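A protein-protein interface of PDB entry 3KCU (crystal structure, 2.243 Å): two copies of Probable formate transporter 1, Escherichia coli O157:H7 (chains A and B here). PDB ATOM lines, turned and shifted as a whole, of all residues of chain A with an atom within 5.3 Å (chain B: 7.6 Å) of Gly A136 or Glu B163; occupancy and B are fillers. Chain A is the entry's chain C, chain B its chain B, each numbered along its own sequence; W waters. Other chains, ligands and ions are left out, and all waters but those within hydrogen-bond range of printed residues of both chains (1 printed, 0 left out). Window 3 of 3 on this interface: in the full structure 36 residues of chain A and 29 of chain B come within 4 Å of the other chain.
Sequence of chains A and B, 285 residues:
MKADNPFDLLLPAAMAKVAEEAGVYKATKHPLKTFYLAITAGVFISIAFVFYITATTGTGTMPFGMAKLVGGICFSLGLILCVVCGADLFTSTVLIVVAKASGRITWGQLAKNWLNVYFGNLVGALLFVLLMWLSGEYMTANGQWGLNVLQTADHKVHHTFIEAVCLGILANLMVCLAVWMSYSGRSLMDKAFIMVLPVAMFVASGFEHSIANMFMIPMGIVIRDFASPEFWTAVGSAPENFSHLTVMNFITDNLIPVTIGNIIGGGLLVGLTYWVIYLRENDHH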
ATOM      1  N   MET A 132       8.490 -32.752 -10.008  1.00  0.00           N
ATOM      2  CA  MET A 132       9.055 -31.611  -9.262  1.00  0.00           C
ATOM      3  C   MET A 132       9.443 -30.490 -10.203  1.00  0.00           C
ATOM      4  O   MET A 132       9.269 -29.323  -9.877  1.00  0.00           O
ATOM      5  CB  MET A 132      10.266 -32.016  -8.400  1.00  0.00           C
ATOM      6  CG  MET A 132       9.934 -32.919  -7.211  1.00  0.00           C
ATOM      7  SD  MET A 132       8.604 -32.234  -6.177  1.00  0.00           S
ATOM      8  CE  MET A 132       9.300 -30.650  -5.660  1.00  0.00           C
ATOM      9  N   TRP A 133       9.969 -30.840 -11.377  1.00  0.00           N
ATOM     10  CA  TRP A 133      10.284 -29.821 -12.371  1.00  0.00           C
ATOM     11  C   TRP A 133       9.026 -29.074 -12.833  1.00  0.00           C
ATOM     12  O   TRP A 133       9.028 -27.845 -12.926  1.00  0.00           O
ATOM     13  CB  TRP A 133      11.022 -30.403 -13.596  1.00  0.00           C
ATOM     14  CG  TRP A 133      11.214 -29.338 -14.632  1.00  0.00           C
ATOM     15  CD1 TRP A 133      10.606 -29.260 -15.845  1.00  0.00           C
ATOM     16  CD2 TRP A 133      12.008 -28.144 -14.499  1.00  0.00           C
ATOM     17  NE1 TRP A 133      10.983 -28.106 -16.488  1.00  0.00           N
ATOM     18  CE2 TRP A 133      11.846 -27.403 -15.685  1.00  0.00           C
ATOM     19  CE3 TRP A 133      12.840 -27.637 -13.489  1.00  0.00           C
ATOM     20  CZ2 TRP A 133      12.489 -26.173 -15.903  1.00  0.00           C
ATOM     21  CZ3 TRP A 133      13.490 -26.415 -13.708  1.00  0.00           C
ATOM     22  CH2 TRP A 133      13.308 -25.701 -14.908  1.00  0.00           C
ATOM     23  N   LEU A 134       7.963 -29.818 -13.143  1.00  0.00           N
ATOM     24  CA  LEU A 134       6.730 -29.201 -13.644  1.00  0.00           C
ATOM     25  C   LEU A 134       5.995 -28.343 -12.597  1.00  0.00           C
ATOM     26  O   LEU A 134       5.255 -27.428 -12.956  1.00  0.00           O
ATOM     27  CB  LEU A 134       5.787 -30.256 -14.229  1.00  0.00           C
ATOM     28  CG  LEU A 134       6.280 -30.921 -15.508  1.00  0.00           C
ATOM     29  CD1 LEU A 134       5.356 -32.087 -15.938  1.00  0.00           C
ATOM     30  CD2 LEU A 134       6.445 -29.869 -16.620  1.00  0.00           C
ATOM     31  N   SER A 135       6.208 -28.635 -11.316  1.00  0.00           N
ATOM     32  CA  SER A 135       5.562 -27.881 -10.241  1.00  0.00           C
ATOM     33  C   SER A 135       6.112 -26.457 -10.093  1.00  0.00           C
ATOM     34  O   SER A 135       5.450 -25.605  -9.494  1.00  0.00           O
ATOM     35  CB  SER A 135       5.699 -28.613  -8.904  1.00  0.00           C
ATOM     36  OG  SER A 135       7.038 -28.557  -8.438  1.00  0.00           O
ATOM     37  N   GLY A 136       7.310 -26.204 -10.628  1.00  0.00           N
ATOM     38  CA  GLY A 136       7.922 -24.877 -10.564  1.00  0.00           C
ATOM     39  C   GLY A 136       8.687 -24.634  -9.257  1.00  0.00           C
ATOM     40  O   GLY A 136       9.244 -23.563  -9.051  1.00  0.00           O
ATOM     41  N   GLU A 137       8.734 -25.660  -8.410  1.00  0.00           N
ATOM     42  CA  GLU A 137       9.345 -25.621  -7.078  1.00  0.00           C
ATOM     43  C   GLU A 137      10.747 -25.017  -6.997  1.00  0.00           C
ATOM     44  O   GLU A 137      11.142 -24.507  -5.951  1.00  0.00           O
ATOM     45  CB  GLU A 137       9.392 -27.040  -6.477  1.00  0.00           C
ATOM     46  CG  GLU A 137       9.778 -27.078  -4.988  1.00  0.00           C
ATOM     47  CD  GLU A 137       8.597 -26.690  -4.079  1.00  0.00           C
ATOM     48  OE1 GLU A 137       8.737 -26.765  -2.838  1.00  0.00           O
ATOM     49  OE2 GLU A 137       7.527 -26.320  -4.616  1.00  0.00           O
ATOM     50  N   TYR A 138      11.514 -25.100  -8.076  1.00  0.00           N
ATOM     51  CA  TYR A 138      12.893 -24.624  -8.032  1.00  0.00           C
ATOM     52  C   TYR A 138      13.005 -23.102  -7.789  1.00  0.00           C
ATOM     53  O   TYR A 138      14.038 -22.623  -7.326  1.00  0.00           O
ATOM     54  CB  TYR A 138      13.669 -25.080  -9.271  1.00  0.00           C
ATOM     55  CG  TYR A 138      13.504 -24.226 -10.509  1.00  0.00           C
ATOM     56  CD1 TYR A 138      12.273 -24.113 -11.145  1.00  0.00           C
ATOM     57  CD2 TYR A 138      14.598 -23.545 -11.059  1.00  0.00           C
ATOM     58  CE1 TYR A 138      12.126 -23.334 -12.306  1.00  0.00           C
ATOM     59  CE2 TYR A 138      14.465 -22.756 -12.213  1.00  0.00           C
ATOM     60  CZ  TYR A 138      13.228 -22.649 -12.825  1.00  0.00           C
ATOM     61  OH  TYR A 138      13.094 -21.885 -13.967  1.00  0.00           O
ATOM     62  N   MET A 139      11.935 -22.360  -8.087  1.00  0.00           N
ATOM     63  CA  MET A 139      11.881 -20.920  -7.811  1.00  0.00           C
ATOM     64  C   MET A 139      11.470 -20.605  -6.356  1.00  0.00           C
ATOM     65  O   MET A 139      11.399 -19.450  -5.990  1.00  0.00           O
ATOM     66  CB  MET A 139      10.926 -20.197  -8.783  1.00  0.00           C
ATOM     67  CG  MET A 139      11.442 -20.124 -10.236  1.00  0.00           C
ATOM     68  SD  MET A 139      13.040 -19.299 -10.304  1.00  0.00           S
ATOM     69  CE  MET A 139      12.608 -17.697  -9.629  1.00  0.00           C
ATOM     70  N   THR A 140      11.223 -21.636  -5.546  1.00  0.00           N
ATOM     71  CA  THR A 140      10.851 -21.449  -4.135  1.00  0.00           C
ATOM     72  C   THR A 140      11.942 -20.686  -3.397  1.00  0.00           C
ATOM     73  O   THR A 140      13.138 -20.922  -3.625  1.00  0.00           O
ATOM     74  CB  THR A 140      10.586 -22.794  -3.425  1.00  0.00           C
ATOM     75  OG1 THR A 140       9.353 -23.336  -3.895  1.00  0.00           O
ATOM     76  CG2 THR A 140      10.529 -22.639  -1.893  1.00  0.00           C
ATOM     77  N   HIS B 158      -0.483 -17.114  -8.055  1.00  0.00           N
ATOM     78  CA  HIS B 158       0.482 -16.728  -9.091  1.00  0.00           C
ATOM     79  C   HIS B 158       1.178 -17.914  -9.752  1.00  0.00           C
ATOM     80  O   HIS B 158       2.204 -17.739 -10.384  1.00  0.00           O
ATOM     81  CB  HIS B 158       1.521 -15.737  -8.547  1.00  0.00           C
ATOM     82  CG  HIS B 158       0.973 -14.365  -8.323  1.00  0.00           C
ATOM     83  ND1 HIS B 158       0.766 -13.839  -7.066  1.00  0.00           N
ATOM     84  CD2 HIS B 158       0.549 -13.424  -9.200  1.00  0.00           C
ATOM     85  CE1 HIS B 158       0.251 -12.627  -7.179  1.00  0.00           C
ATOM     86  NE2 HIS B 158       0.113 -12.350  -8.466  1.00  0.00           N
ATOM     87  N   HIS B 159       0.625 -19.115  -9.601  1.00  0.00           N
ATOM     88  CA  HIS B 159       1.149 -20.282 -10.318  1.00  0.00           C
ATOM     89  C   HIS B 159       0.646 -20.305 -11.769  1.00  0.00           C
ATOM     90  O   HIS B 159      -0.435 -19.777 -12.058  1.00  0.00           O
ATOM     91  CB  HIS B 159       0.727 -21.589  -9.621  1.00  0.00           C
ATOM     92  CG  HIS B 159       1.092 -21.649  -8.169  1.00  0.00           C
ATOM     93  ND1 HIS B 159       2.382 -21.459  -7.717  1.00  0.00           N
ATOM     94  CD2 HIS B 159       0.338 -21.891  -7.065  1.00  0.00           C
ATOM     95  CE1 HIS B 159       2.406 -21.567  -6.398  1.00  0.00           C
ATOM     96  NE2 HIS B 159       1.179 -21.839  -5.978  1.00  0.00           N
ATOM     97  N   THR B 160       1.412 -20.896 -12.688  1.00  0.00           N
ATOM     98  CA  THR B 160       0.806 -21.272 -13.970  1.00  0.00           C
ATOM     99  C   THR B 160      -0.198 -22.399 -13.690  1.00  0.00           C
ATOM    100  O   THR B 160      -0.178 -23.030 -12.620  1.00  0.00           O
ATOM    101  CB  THR B 160       1.822 -21.753 -15.045  1.00  0.00           C
ATOM    102  OG1 THR B 160       2.410 -22.992 -14.641  1.00  0.00           O
ATOM    103  CG2 THR B 160       2.919 -20.697 -15.333  1.00  0.00           C
ATOM    104  N   PHE B 161      -1.085 -22.639 -14.644  1.00  0.00           N
ATOM    105  CA  PHE B 161      -2.062 -23.697 -14.521  1.00  0.00           C
ATOM    106  C   PHE B 161      -1.342 -25.033 -14.300  1.00  0.00           C
ATOM    107  O   PHE B 161      -1.687 -25.794 -13.393  1.00  0.00           O
ATOM    108  CB  PHE B 161      -2.946 -23.751 -15.764  1.00  0.00           C
ATOM    109  CG  PHE B 161      -4.167 -24.614 -15.603  1.00  0.00           C
ATOM    110  CD1 PHE B 161      -5.368 -24.064 -15.186  1.00  0.00           C
ATOM    111  CD2 PHE B 161      -4.113 -25.970 -15.865  1.00  0.00           C
ATOM    112  CE1 PHE B 161      -6.494 -24.852 -15.035  1.00  0.00           C
ATOM    113  CE2 PHE B 161      -5.236 -26.767 -15.709  1.00  0.00           C
ATOM    114  CZ  PHE B 161      -6.426 -26.209 -15.300  1.00  0.00           C
ATOM    115  N   ILE B 162      -0.323 -25.310 -15.107  1.00  0.00           N
ATOM    116  CA  ILE B 162       0.386 -26.574 -14.955  1.00  0.00           C
ATOM    117  C   ILE B 162       1.015 -26.701 -13.566  1.00  0.00           C
ATOM    118  O   ILE B 162       0.904 -27.750 -12.921  1.00  0.00           O
ATOM    119  CB  ILE B 162       1.446 -26.779 -16.044  1.00  0.00           C
ATOM    120  CG1 ILE B 162       0.758 -26.869 -17.404  1.00  0.00           C
ATOM    121  CG2 ILE B 162       2.276 -28.031 -15.749  1.00  0.00           C
ATOM    122  CD1 ILE B 162       1.680 -27.186 -18.560  1.00  0.00           C
ATOM    123  N   GLU B 163       1.667 -25.629 -13.117  1.00  0.00           N
ATOM    124  CA  GLU B 163       2.303 -25.616 -11.809  1.00  0.00           C
ATOM    125  C   GLU B 163       1.277 -25.927 -10.742  1.00  0.00           C
ATOM    126  O   GLU B 163       1.526 -26.746  -9.872  1.00  0.00           O
ATOM    127  CB  GLU B 163       2.960 -24.249 -11.518  1.00  0.00           C
ATOM    128  CG  GLU B 163       4.286 -24.038 -12.241  1.00  0.00           C
ATOM    129  CD  GLU B 163       4.765 -22.578 -12.220  1.00  0.00           C
ATOM    130  OE1 GLU B 163       5.950 -22.347 -12.530  1.00  0.00           O
ATOM    131  OE2 GLU B 163       3.963 -21.662 -11.918  1.00  0.00           O
ATOM    132  N   ALA B 164       0.121 -25.272 -10.819  1.00  0.00           N
ATOM    133  CA  ALA B 164      -0.884 -25.411  -9.775  1.00  0.00           C
ATOM    134  C   ALA B 164      -1.409 -26.846  -9.751  1.00  0.00           C
ATOM    135  O   ALA B 164      -1.555 -27.432  -8.682  1.00  0.00           O
ATOM    136  CB  ALA B 164      -2.017 -24.384  -9.949  1.00  0.00           C
ATOM    137  N   VAL B 165      -1.644 -27.425 -10.928  1.00  0.00           N
ATOM    138  CA  VAL B 165      -2.018 -28.845 -11.013  1.00  0.00           C
ATOM    139  C   VAL B 165      -0.960 -29.757 -10.383  1.00  0.00           C
ATOM    140  O   VAL B 165      -1.286 -30.653  -9.611  1.00  0.00           O
ATOM    141  CB  VAL B 165      -2.295 -29.293 -12.478  1.00  0.00           C
ATOM    142  CG1 VAL B 165      -2.473 -30.842 -12.571  1.00  0.00           C
ATOM    143  CG2 VAL B 165      -3.514 -28.568 -13.023  1.00  0.00           C
ATOM    144  N   CYS B 166       0.310 -29.522 -10.701  1.00  0.00           N
ATOM    145  CA  CYS B 166       1.368 -30.375 -10.173  1.00  0.00           C
ATOM    146  C   CYS B 166       1.533 -30.202  -8.666  1.00  0.00           C
ATOM    147  O   CYS B 166       1.692 -31.186  -7.944  1.00  0.00           O
ATOM    148  CB  CYS B 166       2.690 -30.159 -10.931  1.00  0.00           C
ATOM    149  SG  CYS B 166       2.627 -30.798 -12.672  1.00  0.00           S
ATOM    150  N   LEU B 167       1.477 -28.954  -8.197  1.00  0.00           N
ATOM    151  CA  LEU B 167       1.490 -28.683  -6.757  1.00  0.00           C
ATOM    152  C   LEU B 167       0.291 -29.342  -6.050  1.00  0.00           C
ATOM    153  O   LEU B 167       0.400 -29.792  -4.911  1.00  0.00           O
ATOM    154  CB  LEU B 167       1.536 -27.165  -6.497  1.00  0.00           C
ATOM    155  CG  LEU B 167       2.845 -26.489  -6.948  1.00  0.00           C
ATOM    156  CD1 LEU B 167       2.735 -24.961  -6.997  1.00  0.00           C
ATOM    157  CD2 LEU B 167       4.026 -26.923  -6.083  1.00  0.00           C
ATOM    158  N   GLY B 168      -0.841 -29.410  -6.752  1.00  0.00           N
ATOM    159  CA  GLY B 168      -2.026 -30.078  -6.264  1.00  0.00           C
ATOM    160  C   GLY B 168      -1.854 -31.594  -6.226  1.00  0.00           C
ATOM    161  O   GLY B 168      -2.307 -32.261  -5.291  1.00  0.00           O
ATOM    162  N   ILE B 169      -1.187 -32.142  -7.239  1.00  0.00           N
ATOM    163  CA  ILE B 169      -0.861 -33.554  -7.223  1.00  0.00           C
ATOM    164  C   ILE B 169       0.027 -33.853  -6.033  1.00  0.00           C
ATOM    165  O   ILE B 169      -0.189 -34.824  -5.310  1.00  0.00           O
ATOM    166  CB  ILE B 169      -0.122 -33.989  -8.498  1.00  0.00           C
ATOM    167  CG1 ILE B 169      -1.049 -33.889  -9.717  1.00  0.00           C
ATOM    168  CG2 ILE B 169       0.397 -35.430  -8.351  1.00  0.00           C
ATOM    169  CD1 ILE B 169      -0.310 -34.034 -11.066  1.00  0.00           C
ATOM    170  N   LEU B 170       1.031 -33.003  -5.833  1.00  0.00           N
ATOM    171  CA  LEU B 170       2.009 -33.231  -4.783  1.00  0.00           C
ATOM    172  C   LEU B 170       1.397 -33.187  -3.375  1.00  0.00           C
ATOM    173  O   LEU B 170       1.704 -34.031  -2.540  1.00  0.00           O
ATOM    174  CB  LEU B 170       3.162 -32.249  -4.921  1.00  0.00           C
ATOM    175  CG  LEU B 170       4.118 -32.595  -6.075  1.00  0.00           C
ATOM    176  CD1 LEU B 170       4.909 -31.371  -6.511  1.00  0.00           C
ATOM    177  CD2 LEU B 170       5.058 -33.704  -5.644  1.00  0.00           C
ATOM    178  N   GLU B 208      -0.014 -27.630  -2.819  1.00  0.00           N
ATOM    179  CA  GLU B 208      -1.314 -26.972  -2.852  1.00  0.00           C
ATOM    180  C   GLU B 208      -2.455 -27.949  -2.566  1.00  0.00           C
ATOM    181  O   GLU B 208      -2.696 -28.906  -3.325  1.00  0.00           O
ATOM    182  CB  GLU B 208      -1.523 -26.291  -4.216  1.00  0.00           C
ATOM    183  CG  GLU B 208      -0.617 -25.089  -4.492  1.00  0.00           C
ATOM    184  CD  GLU B 208      -1.049 -23.831  -3.739  1.00  0.00           C
ATOM    185  OE1 GLU B 208      -2.034 -23.880  -2.963  1.00  0.00           O
ATOM    186  OE2 GLU B 208      -0.390 -22.790  -3.925  1.00  0.00           O
ATOM    187  N   ASP B 253      -7.355 -19.485 -10.958  1.00  0.00           N
ATOM    188  CA  ASP B 253      -5.905 -19.603 -10.932  1.00  0.00           C
ATOM    189  C   ASP B 253      -5.399 -20.546  -9.845  1.00  0.00           C
ATOM    190  O   ASP B 253      -4.233 -20.940  -9.845  1.00  0.00           O
ATOM    191  CB  ASP B 253      -5.263 -18.219 -10.802  1.00  0.00           C
ATOM    192  CG  ASP B 253      -5.605 -17.305 -11.977  1.00  0.00           C
ATOM    193  OD1 ASP B 253      -5.633 -16.066 -11.790  1.00  0.00           O
ATOM    194  OD2 ASP B 253      -5.854 -17.834 -13.089  1.00  0.00           O
ATOM    195  N   PRO B 257      -7.355 -25.621 -10.867  1.00  0.00           N
ATOM    196  CA  PRO B 257      -6.142 -26.399 -11.166  1.00  0.00           C
ATOM    197  C   PRO B 257      -5.644 -27.230  -9.974  1.00  0.00           C
ATOM    198  O   PRO B 257      -5.190 -28.363 -10.149  1.00  0.00           O
ATOM    199  CB  PRO B 257      -5.096 -25.329 -11.527  1.00  0.00           C
ATOM    200  CG  PRO B 257      -5.850 -24.057 -11.703  1.00  0.00           C
ATOM    201  CD  PRO B 257      -7.138 -24.168 -10.973  1.00  0.00           C
ATOM    202  N   VAL B 258      -5.706 -26.659  -8.775  1.00  0.00           N
ATOM    203  CA  VAL B 258      -5.281 -27.374  -7.576  1.00  0.00           C
ATOM    204  C   VAL B 258      -6.196 -28.584  -7.279  1.00  0.00           C
ATOM    205  O   VAL B 258      -5.723 -29.684  -6.967  1.00  0.00           O
ATOM    206  CB  VAL B 258      -5.198 -26.400  -6.363  1.00  0.00           C
ATOM    207  CG1 VAL B 258      -5.064 -27.153  -5.017  1.00  0.00           C
ATOM    208  CG2 VAL B 258      -4.053 -25.403  -6.570  1.00  0.00           C
HETATM  209  O   HOH W   1       8.162 -21.452 -10.656  1.00  0.00           O
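No position is printed for both chains. Of the 9 pairs that touch across the chains among the printed residues, none has its exchanged pair printed and touching as well.
Gly A136 touches just one residue of chain B: Glu B163. Glu B163 touches just these residues of chain A: Leu A134, Ser A135 and Gly A136. Printed residues of chain B within 4 Å of Ser A135: Glu B163, Cys B166, Leu B167 and Leu B170. Of the printed residues of chain A, Leu B170 touches Met A132 and Ser A135. Printed residues of chain A within 4 Å of Leu B167: Ser A135 and Glu A137. Of the printed residues of chain B, Glu A137 touches Leu B167. Printed residues of chain A within 4 Å of Cys B166: Leu A134 (3.6 Å) and Ser A135 (3.7 Å). Of the printed residues of chain B, Met A132 touches Leu B170 (3.8 Å). Thr B160 touches none of the printed residues of chain A. Thr A140 touches none of the printed residues of chain B. The nearest residue of chain B that does not touch Gly A136 is Leu B167 (5.7 Å). The nearest printed residue of chain B that does not touch Met A132 is Cys B166 (6.4 Å).
Hydrophobic or aromatic side chains of chain B within 4 Å of the printed part of chain A: Leu B167 and Leu B170. Along chain B the printed residues that touch a printed residue of chain A span positions 163 to 170. Of the 9 printed residues of chain A, 5 touch a printed residue of chain B. Printed residues of chain A that touch a printed residue of chain B: Met A132, Leu A134, Ser A135, Gly A136 and Glu A137. Among the printed residues, 9 pairs touch across the chains.
Water W1 lies within hydrogen-bond range of O of Gly A136 (2.9 Å) and OE1 of Glu B163 (3.0 Å).
O of Ile B162 is in hydrogen-bond range of SG of Cys B166, 3.5 Å away. The backbone carbonyl oxygen (O) of Glu A137 is in hydrogen-bond range of the side-chain hydroxyl (OG1) of Thr A140. N of Thr B160 sits at hydrogen-bond distance from OE2 of Glu B163, at 2.8 Å. The backbone NH of Glu B208 sits at hydrogen-bond distance from the backbone carbonyl oxygen of Leu B167. The side-chain hydroxyl (OG) of Ser A135 sits close to the backbone NH (N) of Glu A137 (3.4 Å). O of Met A132 is in hydrogen-bond range of OG of Ser A135 (2.8 Å).
Among the printed residues, pairs that only touch across the chains: Met A132 with Leu B170, Leu A134 with Glu B163, Leu A134 with Cys B166, Ser A135 with Glu B163, Ser A135 with Cys B166, Ser A135 with Leu B167, Ser A135 with Leu B170, Gly A136 with Glu B163 and Glu A137 with Leu B167.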
